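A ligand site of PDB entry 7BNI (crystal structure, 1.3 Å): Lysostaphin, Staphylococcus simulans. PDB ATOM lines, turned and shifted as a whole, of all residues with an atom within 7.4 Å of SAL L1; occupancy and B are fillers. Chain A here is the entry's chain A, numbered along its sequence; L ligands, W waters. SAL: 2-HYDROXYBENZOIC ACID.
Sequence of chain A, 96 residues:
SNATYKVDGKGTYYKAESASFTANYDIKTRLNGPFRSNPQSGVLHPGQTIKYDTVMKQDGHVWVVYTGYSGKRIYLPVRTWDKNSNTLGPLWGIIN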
ATOM      1  N   ASN A   2     -25.899  -2.344  18.463  1.00  0.00           N
ATOM      2  CA  ASN A   2     -24.796  -2.170  17.502  1.00  0.00           C
ATOM      3  C   ASN A   2     -25.291  -1.548  16.203  1.00  0.00           C
ATOM      4  O   ASN A   2     -24.932  -1.970  15.097  1.00  0.00           O
ATOM      5  CB  ASN A   2     -24.089  -3.509  17.274  1.00  0.00           C
ATOM      6  CG  ASN A   2     -23.558  -4.096  18.560  1.00  0.00           C
ATOM      7  OD1 ASN A   2     -24.080  -5.084  19.062  1.00  0.00           O
ATOM      8  ND2 ASN A   2     -22.518  -3.493  19.100  1.00  0.00           N
ATOM      9  N   THR A   4     -24.556   1.087  14.672  1.00  0.00           N
ATOM     10  CA  THR A   4     -23.542   1.674  13.786  1.00  0.00           C
ATOM     11  C   THR A   4     -22.629   0.631  13.151  1.00  0.00           C
ATOM     12  O   THR A   4     -21.720   0.983  12.378  1.00  0.00           O
ATOM     13  CB  THR A   4     -22.690   2.673  14.569  1.00  0.00           C
ATOM     14  OG1 THR A   4     -21.978   1.973  15.607  1.00  0.00           O
ATOM     15  CG2 THR A   4     -23.563   3.765  15.175  1.00  0.00           C
ATOM     16  N   TYR A   5     -22.830  -0.645  13.464  1.00  0.00           N
ATOM     17  CA  TYR A   5     -22.064  -1.727  12.880  1.00  0.00           C
ATOM     18  C   TYR A   5     -22.904  -2.418  11.826  1.00  0.00           C
ATOM     19  O   TYR A   5     -24.133  -2.379  11.875  1.00  0.00           O
ATOM     20  CB  TYR A   5     -21.698  -2.739  13.975  1.00  0.00           C
ATOM     21  CG  TYR A   5     -20.690  -2.286  14.999  1.00  0.00           C
ATOM     22  CD1 TYR A   5     -21.032  -1.444  16.045  1.00  0.00           C
ATOM     23  CD2 TYR A   5     -19.377  -2.721  14.913  1.00  0.00           C
ATOM     24  CE1 TYR A   5     -20.088  -1.038  16.968  1.00  0.00           C
ATOM     25  CE2 TYR A   5     -18.433  -2.337  15.811  1.00  0.00           C
ATOM     26  CZ  TYR A   5     -18.780  -1.499  16.845  1.00  0.00           C
ATOM     27  OH  TYR A   5     -17.802  -1.131  17.741  1.00  0.00           O
ATOM     28  N   LYS A  15     -17.177  -2.428  11.603  1.00  0.00           N
ATOM     29  CA  LYS A  15     -17.305  -1.056  11.127  1.00  0.00           C
ATOM     30  C   LYS A  15     -15.913  -0.514  10.815  1.00  0.00           C
ATOM     31  O   LYS A  15     -14.929  -0.895  11.440  1.00  0.00           O
ATOM     32  CB  LYS A  15     -18.019  -0.152  12.150  1.00  0.00           C
ATOM     33  CG  LYS A  15     -17.244   0.029  13.427  1.00  0.00           C
ATOM     34  CD  LYS A  15     -17.905   1.019  14.385  1.00  0.00           C
ATOM     35  CE  LYS A  15     -17.097   1.185  15.660  1.00  0.00           C
ATOM     36  NZ  LYS A  15     -17.469   2.382  16.455  1.00  0.00           N
ATOM     37  N   GLU A  17     -13.225   2.176  11.090  1.00  0.00           N
ATOM     38  CA  GLU A  17     -12.868   3.227  12.027  1.00  0.00           C
ATOM     39  C   GLU A  17     -11.371   3.130  12.263  1.00  0.00           C
ATOM     40  O   GLU A  17     -10.838   2.022  12.409  1.00  0.00           O
ATOM     41  CB  GLU A  17     -13.669   3.040  13.314  1.00  0.00           C
ATOM     42  CG  GLU A  17     -13.513   4.159  14.311  1.00  0.00           C
ATOM     43  CD  GLU A  17     -14.477   4.017  15.459  1.00  0.00           C
ATOM     44  OE1 GLU A  17     -14.118   3.678  16.567  1.00  0.00           O
ATOM     45  OE2 GLU A  17     -15.671   4.278  15.193  1.00  0.00           O
ATOM     46  N   ALA A  19      -7.812   4.557  14.193  1.00  0.00           N
ATOM     47  CA  ALA A  19      -7.099   5.278  15.237  1.00  0.00           C
ATOM     48  C   ALA A  19      -5.878   4.438  15.586  1.00  0.00           C
ATOM     49  O   ALA A  19      -5.573   3.458  14.898  1.00  0.00           O
ATOM     50  CB  ALA A  19      -7.987   5.540  16.453  1.00  0.00           C
ATOM     51  N   PHE A  21      -3.810   2.307  18.743  1.00  0.00           N
ATOM     52  CA  PHE A  21      -3.985   1.607  20.006  1.00  0.00           C
ATOM     53  C   PHE A  21      -2.612   1.268  20.540  1.00  0.00           C
ATOM     54  O   PHE A  21      -1.805   0.663  19.831  1.00  0.00           O
ATOM     55  CB  PHE A  21      -4.799   0.316  19.827  1.00  0.00           C
ATOM     56  CG  PHE A  21      -4.923  -0.487  21.089  1.00  0.00           C
ATOM     57  CD1 PHE A  21      -5.962  -0.229  21.980  1.00  0.00           C
ATOM     58  CD2 PHE A  21      -4.028  -1.499  21.391  1.00  0.00           C
ATOM     59  CE1 PHE A  21      -6.096  -0.962  23.146  1.00  0.00           C
ATOM     60  CE2 PHE A  21      -4.154  -2.220  22.589  1.00  0.00           C
ATOM     61  CZ  PHE A  21      -5.193  -1.951  23.453  1.00  0.00           C
ATOM     62  N   TYR A  52      -5.017   0.900  13.544  1.00  0.00           N
ATOM     63  CA  TYR A  52      -6.091   0.027  13.081  1.00  0.00           C
ATOM     64  C   TYR A  52      -7.041   0.765  12.148  1.00  0.00           C
ATOM     65  O   TYR A  52      -7.116   1.989  12.132  1.00  0.00           O
ATOM     66  CB  TYR A  52      -6.860  -0.594  14.253  1.00  0.00           C
ATOM     67  CG  TYR A  52      -7.568   0.362  15.171  1.00  0.00           C
ATOM     68  CD1 TYR A  52      -8.856   0.814  14.893  1.00  0.00           C
ATOM     69  CD2 TYR A  52      -6.976   0.743  16.359  1.00  0.00           C
ATOM     70  CE1 TYR A  52      -9.512   1.654  15.781  1.00  0.00           C
ATOM     71  CE2 TYR A  52      -7.600   1.590  17.222  1.00  0.00           C
ATOM     72  CZ  TYR A  52      -8.880   2.033  16.951  1.00  0.00           C
ATOM     73  OH  TYR A  52      -9.512   2.839  17.866  1.00  0.00           O
ATOM     74  N   THR A  54     -10.355  -1.059  11.269  1.00  0.00           N
ATOM     75  CA  THR A  54     -11.643  -1.726  11.364  1.00  0.00           C
ATOM     76  C   THR A  54     -11.813  -2.138  12.813  1.00  0.00           C
ATOM     77  O   THR A  54     -10.829  -2.498  13.463  1.00  0.00           O
ATOM     78  CB  THR A  54     -11.672  -2.955  10.449  1.00  0.00           C
ATOM     79  OG1 THR A  54     -11.413  -2.561   9.106  1.00  0.00           O
ATOM     80  CG2 THR A  54     -13.035  -3.626  10.490  1.00  0.00           C
ATOM     81  N   VAL A  55     -13.051  -2.050  13.309  1.00  0.00           N
ATOM     82  CA  VAL A  55     -13.426  -2.475  14.653  1.00  0.00           C
ATOM     83  C   VAL A  55     -14.469  -3.588  14.505  1.00  0.00           C
ATOM     84  O   VAL A  55     -15.383  -3.470  13.691  1.00  0.00           O
ATOM     85  CB  VAL A  55     -14.005  -1.318  15.484  1.00  0.00           C
ATOM     86  CG1 VAL A  55     -14.399  -1.774  16.905  1.00  0.00           C
ATOM     87  CG2 VAL A  55     -13.037  -0.149  15.513  1.00  0.00           C
ATOM     88  N   MET A  56     -14.332  -4.645  15.287  1.00  0.00           N
ATOM     89  CA  MET A  56     -15.247  -5.787  15.255  1.00  0.00           C
ATOM     90  C   MET A  56     -15.659  -6.163  16.655  1.00  0.00           C
ATOM     91  O   MET A  56     -14.910  -5.993  17.618  1.00  0.00           O
ATOM     92  CB  MET A  56     -14.516  -6.937  14.581  1.00  0.00           C
ATOM     93  CG  MET A  56     -14.046  -6.610  13.182  1.00  0.00           C
ATOM     94  SD  MET A  56     -13.507  -8.116  12.344  1.00  0.00           S
ATOM     95  CE  MET A  56     -13.287  -7.505  10.657  1.00  0.00           C
ATOM     96  N   LYS A  57     -16.848  -6.728  16.756  1.00  0.00           N
ATOM     97  CA  LYS A  57     -17.320  -7.342  17.993  1.00  0.00           C
ATOM     98  C   LYS A  57     -17.678  -8.785  17.725  1.00  0.00           C
ATOM     99  O   LYS A  57     -18.570  -9.078  16.925  1.00  0.00           O
ATOM    100  CB  LYS A  57     -18.465  -6.569  18.632  1.00  0.00           C
ATOM    101  CG  LYS A  57     -18.249  -5.083  18.736  1.00  0.00           C
ATOM    102  CD  LYS A  57     -19.502  -4.392  19.309  1.00  0.00           C
ATOM    103  CE  LYS A  57     -19.210  -3.065  19.982  1.00  0.00           C
ATOM    104  NZ  LYS A  57     -20.443  -2.337  20.415  1.00  0.00           N
ATOM    105  N   VAL A  62     -14.390  -6.621  21.954  1.00  0.00           N
ATOM    106  CA  VAL A  62     -14.144  -5.696  20.853  1.00  0.00           C
ATOM    107  C   VAL A  62     -12.737  -5.951  20.366  1.00  0.00           C
ATOM    108  O   VAL A  62     -11.811  -6.113  21.183  1.00  0.00           O
ATOM    109  CB  VAL A  62     -14.279  -4.224  21.275  1.00  0.00           C
ATOM    110  CG1 VAL A  62     -14.198  -3.313  20.051  1.00  0.00           C
ATOM    111  CG2 VAL A  62     -15.582  -4.000  22.022  1.00  0.00           C
ATOM    112  N   TRP A  63     -12.561  -5.982  19.057  1.00  0.00           N
ATOM    113  CA  TRP A  63     -11.305  -6.216  18.377  1.00  0.00           C
ATOM    114  C   TRP A  63     -11.037  -5.034  17.450  1.00  0.00           C
ATOM    115  O   TRP A  63     -11.966  -4.453  16.897  1.00  0.00           O
ATOM    116  CB  TRP A  63     -11.316  -7.485  17.501  1.00  0.00           C
ATOM    117  CG  TRP A  63     -11.742  -8.722  18.209  1.00  0.00           C
ATOM    118  CD1 TRP A  63     -12.981  -9.010  18.692  1.00  0.00           C
ATOM    119  CD2 TRP A  63     -10.911  -9.851  18.504  1.00  0.00           C
ATOM    120  NE1 TRP A  63     -12.977 -10.282  19.245  1.00  0.00           N
ATOM    121  CE2 TRP A  63     -11.721 -10.810  19.131  1.00  0.00           C
ATOM    122  CE3 TRP A  63      -9.589 -10.176  18.215  1.00  0.00           C
ATOM    123  CZ2 TRP A  63     -11.221 -12.040  19.568  1.00  0.00           C
ATOM    124  CZ3 TRP A  63      -9.095 -11.401  18.613  1.00  0.00           C
ATOM    125  CH2 TRP A  63      -9.902 -12.312  19.277  1.00  0.00           C
ATOM    126  N   VAL A  64      -9.756  -4.742  17.243  1.00  0.00           N
ATOM    127  CA  VAL A  64      -9.348  -3.832  16.172  1.00  0.00           C
ATOM    128  C   VAL A  64      -8.486  -4.613  15.190  1.00  0.00           C
ATOM    129  O   VAL A  64      -7.859  -5.620  15.541  1.00  0.00           O
ATOM    130  CB  VAL A  64      -8.630  -2.575  16.681  1.00  0.00           C
ATOM    131  CG1 VAL A  64      -9.539  -1.847  17.655  1.00  0.00           C
ATOM    132  CG2 VAL A  64      -7.277  -2.901  17.319  1.00  0.00           C
ATOM    133  N   VAL A  78      -9.269  -5.827  22.444  1.00  0.00           N
ATOM    134  CA  VAL A  78      -8.927  -4.642  23.205  1.00  0.00           C
ATOM    135  C   VAL A  78      -9.746  -4.462  24.477  1.00  0.00           C
ATOM    136  O   VAL A  78      -9.353  -3.635  25.334  1.00  0.00           O
ATOM    137  CB  VAL A  78      -8.933  -3.345  22.378  1.00  0.00           C
ATOM    138  CG1 VAL A  78      -7.929  -3.450  21.198  1.00  0.00           C
ATOM    139  CG2 VAL A  78     -10.326  -2.994  21.866  1.00  0.00           C
ATOM    140  N   ARG A  79     -10.846  -5.180  24.653  1.00  0.00           N
ATOM    141  CA  ARG A  79     -11.689  -5.130  25.845  1.00  0.00           C
ATOM    142  C   ARG A  79     -12.782  -6.180  25.705  1.00  0.00           C
ATOM    143  O   ARG A  79     -13.059  -6.673  24.610  1.00  0.00           O
ATOM    144  CB  ARG A  79     -12.344  -3.754  26.018  1.00  0.00           C
ATOM    145  CG  ARG A  79     -13.440  -3.491  24.987  1.00  0.00           C
ATOM    146  CD  ARG A  79     -13.646  -2.013  24.689  1.00  0.00           C
ATOM    147  NE  ARG A  79     -13.905  -1.283  25.929  1.00  0.00           N
ATOM    148  CZ  ARG A  79     -14.079   0.016  26.013  1.00  0.00           C
ATOM    149  NH1 ARG A  79     -14.047   0.798  24.935  1.00  0.00           N
ATOM    150  NH2 ARG A  79     -14.266   0.547  27.212  1.00  0.00           N
ATOM    151  N   THR A  80     -13.421  -6.489  26.822  1.00  0.00           N
ATOM    152  CA  THR A  80     -14.534  -7.434  26.744  1.00  0.00           C
ATOM    153  C   THR A  80     -15.793  -6.753  26.216  1.00  0.00           C
ATOM    154  O   THR A  80     -15.948  -5.524  26.294  1.00  0.00           O
ATOM    155  CB  THR A  80     -14.857  -8.026  28.117  1.00  0.00           C
ATOM    156  OG1 THR A  80     -15.234  -6.986  29.031  1.00  0.00           O
ATOM    157  CG2 THR A  80     -13.671  -8.794  28.678  1.00  0.00           C
ATOM    158  N   ASN A  86     -24.522  -5.432  25.177  1.00  0.00           N
ATOM    159  CA  ASN A  86     -23.591  -4.464  24.598  1.00  0.00           C
ATOM    160  C   ASN A  86     -22.719  -3.776  25.655  1.00  0.00           C
ATOM    161  O   ASN A  86     -22.160  -2.698  25.398  1.00  0.00           O
ATOM    162  CB  ASN A  86     -24.282  -3.433  23.698  1.00  0.00           C
ATOM    163  CG  ASN A  86     -23.358  -2.932  22.589  1.00  0.00           C
ATOM    164  OD1 ASN A  86     -22.259  -3.443  22.376  1.00  0.00           O
ATOM    165  ND2 ASN A  86     -23.810  -1.902  21.899  1.00  0.00           N
ATOM    166  N   LEU A  88     -19.406  -3.059  27.754  1.00  0.00           N
ATOM    167  CA  LEU A  88     -17.987  -3.128  27.422  1.00  0.00           C
ATOM    168  C   LEU A  88     -17.161  -3.073  28.698  1.00  0.00           C
ATOM    169  O   LEU A  88     -17.494  -2.344  29.634  1.00  0.00           O
ATOM    170  CB  LEU A  88     -17.576  -1.951  26.570  1.00  0.00           C
ATOM    171  CG  LEU A  88     -18.260  -1.809  25.202  1.00  0.00           C
ATOM    172  CD1 LEU A  88     -17.702  -0.578  24.458  1.00  0.00           C
ATOM    173  CD2 LEU A  88     -18.085  -3.055  24.371  1.00  0.00           C
ATOM    174  N   GLY A  89     -16.091  -3.875  28.716  1.00  0.00           N
ATOM    175  CA  GLY A  89     -15.147  -3.824  29.807  1.00  0.00           C
ATOM    176  C   GLY A  89     -14.116  -2.738  29.606  1.00  0.00           C
ATOM    177  O   GLY A  89     -14.086  -2.035  28.600  1.00  0.00           O
ATOM    178  N   LEU A  91     -10.797  -0.766  28.711  1.00  0.00           N
ATOM    179  CA  LEU A  91      -9.839  -0.913  27.625  1.00  0.00           C
ATOM    180  C   LEU A  91      -8.484  -1.388  28.121  1.00  0.00           C
ATOM    181  O   LEU A  91      -8.003  -0.977  29.176  1.00  0.00           O
ATOM    182  CB  LEU A  91      -9.655   0.435  26.939  1.00  0.00           C
ATOM    183  CG  LEU A  91     -10.478   0.693  25.682  1.00  0.00           C
ATOM    184  CD1 LEU A  91     -10.387   2.167  25.371  1.00  0.00           C
ATOM    185  CD2 LEU A  91      -9.999  -0.122  24.529  1.00  0.00           C
ATOM    186  N   ILE A  95      -6.191   4.579  23.387  1.00  0.00           N
ATOM    187  CA  ILE A  95      -6.560   4.933  22.031  1.00  0.00           C
ATOM    188  C   ILE A  95      -6.289   6.417  21.862  1.00  0.00           C
ATOM    189  O   ILE A  95      -6.716   7.241  22.691  1.00  0.00           O
ATOM    190  CB  ILE A  95      -8.023   4.564  21.733  1.00  0.00           C
ATOM    191  CG1 ILE A  95      -8.180   3.039  21.756  1.00  0.00           C
ATOM    192  CG2 ILE A  95      -8.461   5.134  20.376  1.00  0.00           C
ATOM    193  CD1 ILE A  95      -9.556   2.466  21.461  1.00  0.00           C
HETATM  194  C1' SAL L   1     -16.220   1.028  20.187  1.00  0.00           C
HETATM  195  O1' SAL L   1     -16.798   1.642  19.259  1.00  0.00           O
HETATM  196  O2' SAL L   1     -16.847   0.602  21.186  1.00  0.00           O
HETATM  197  C1  SAL L   1     -14.723   0.841  20.086  1.00  0.00           C
HETATM  198  C2  SAL L   1     -14.045   0.382  21.197  1.00  0.00           C
HETATM  199  C3  SAL L   1     -12.677   0.219  21.172  1.00  0.00           C
HETATM  200  C4  SAL L   1     -11.976   0.471  20.014  1.00  0.00           C
HETATM  201  C5  SAL L   1     -12.653   0.939  18.899  1.00  0.00           C
HETATM  202  C6  SAL L   1     -14.018   1.120  18.941  1.00  0.00           C
HETATM  203  O2  SAL L   1     -14.772   0.115  22.339  1.00  0.00           O
HETATM  204  C1' SAL L   2     -22.254   5.793  19.118  1.00  0.00           C
HETATM  205  O1' SAL L   2     -21.105   5.553  18.679  1.00  0.00           O
HETATM  206  O2' SAL L   2     -22.544   5.571  20.319  1.00  0.00           O
HETATM  207  C1  SAL L   2     -23.292   6.346  18.164  1.00  0.00           C
HETATM  208  C2  SAL L   2     -24.583   6.499  18.595  1.00  0.00           C
HETATM  209  C3  SAL L   2     -25.556   6.986  17.759  1.00  0.00           C
HETATM  210  C4  SAL L   2     -25.238   7.329  16.466  1.00  0.00           C
HETATM  211  C5  SAL L   2     -23.947   7.145  16.014  1.00  0.00           C
HETATM  212  C6  SAL L   2     -22.979   6.653  16.862  1.00  0.00           C
HETATM  213  O2  SAL L   2     -24.861   6.176  19.920  1.00  0.00           O
HETATM  214  O   HOH W   1     -19.401  -0.147  20.683  1.00  0.00           O
HETATM  215  O   HOH W   2     -18.127   4.268  20.868  1.00  0.00           O
HETATM  216  O   HOH W   3     -20.158   2.141  19.412  1.00  0.00           O
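The backbone carbonyl oxygen (O) of Arg 79 is in hydrogen-bond range of the backbone NH (N) of Val 62, at 3.0 Å.
The backbone carbonyl oxygen (O) of Gly 89 lies within hydrogen-bond range of the guanidinium group (NE) of Arg 79, at 2.8 Å.
The side-chain amino group (NZ) of Lys 15 is in salt-bridge range of the side-chain carboxylate (OE2) of Glu 17, 2.9 Å away.
N of Val 55 is in hydrogen-bond range of O of Lys 15, at 2.9 Å.
The backbone NH of Thr 54 lies within hydrogen-bond range of the backbone carbonyl oxygen of Glu 17 (3.3 Å).
The backbone carbonyl oxygen (O) of Ala 19 lies within hydrogen-bond range of the backbone NH (N) of Tyr 52 (2.9 Å).
The backbone carbonyl oxygen (O) of Val 62 sits at hydrogen-bond distance from the backbone NH (N) of Val 78 (2.9 Å).
An oxygen (O2) of SAL L1 lies within hydrogen-bond range of the guanidinium group (NH1) of Arg 79, at 2.8 Å.
O1' of SAL L1 lies within salt-bridge range of NZ of Lys 15 (3.0 Å).
The side-chain hydroxyl (OH) of Tyr 5 lies within hydrogen-bond range of an oxygen (O1') of SAL L1, at 3.3 Å.
Water W1 lies within hydrogen-bond range of NZ of Lys 57 (2.4 Å), O2' of SAL L1 (2.7 Å) and OH of Tyr 5 (3.5 Å).
Residues that only touch SAL L1: Glu 17 (3.5 Å), Tyr 52 (3.8 Å), Val 55 (3.6 Å), Val 62 (3.9 Å), Leu 88 (3.6 Å) and Ile 95 (3.5 Å).
Hydrophobic or aromatic side chains within 4 Å of SAL L1: Val 55, Val 62, Leu 88 and Ile 95.
Nine residues have an atom within 4 Å of SAL L1: Tyr 5, Lys 15, Glu 17, Tyr 52, Val 55, Val 62, Arg 79, Leu 88 and Ile 95.
Along chain A the residues within 4 Å of SAL L1 span positions 5 to 95.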
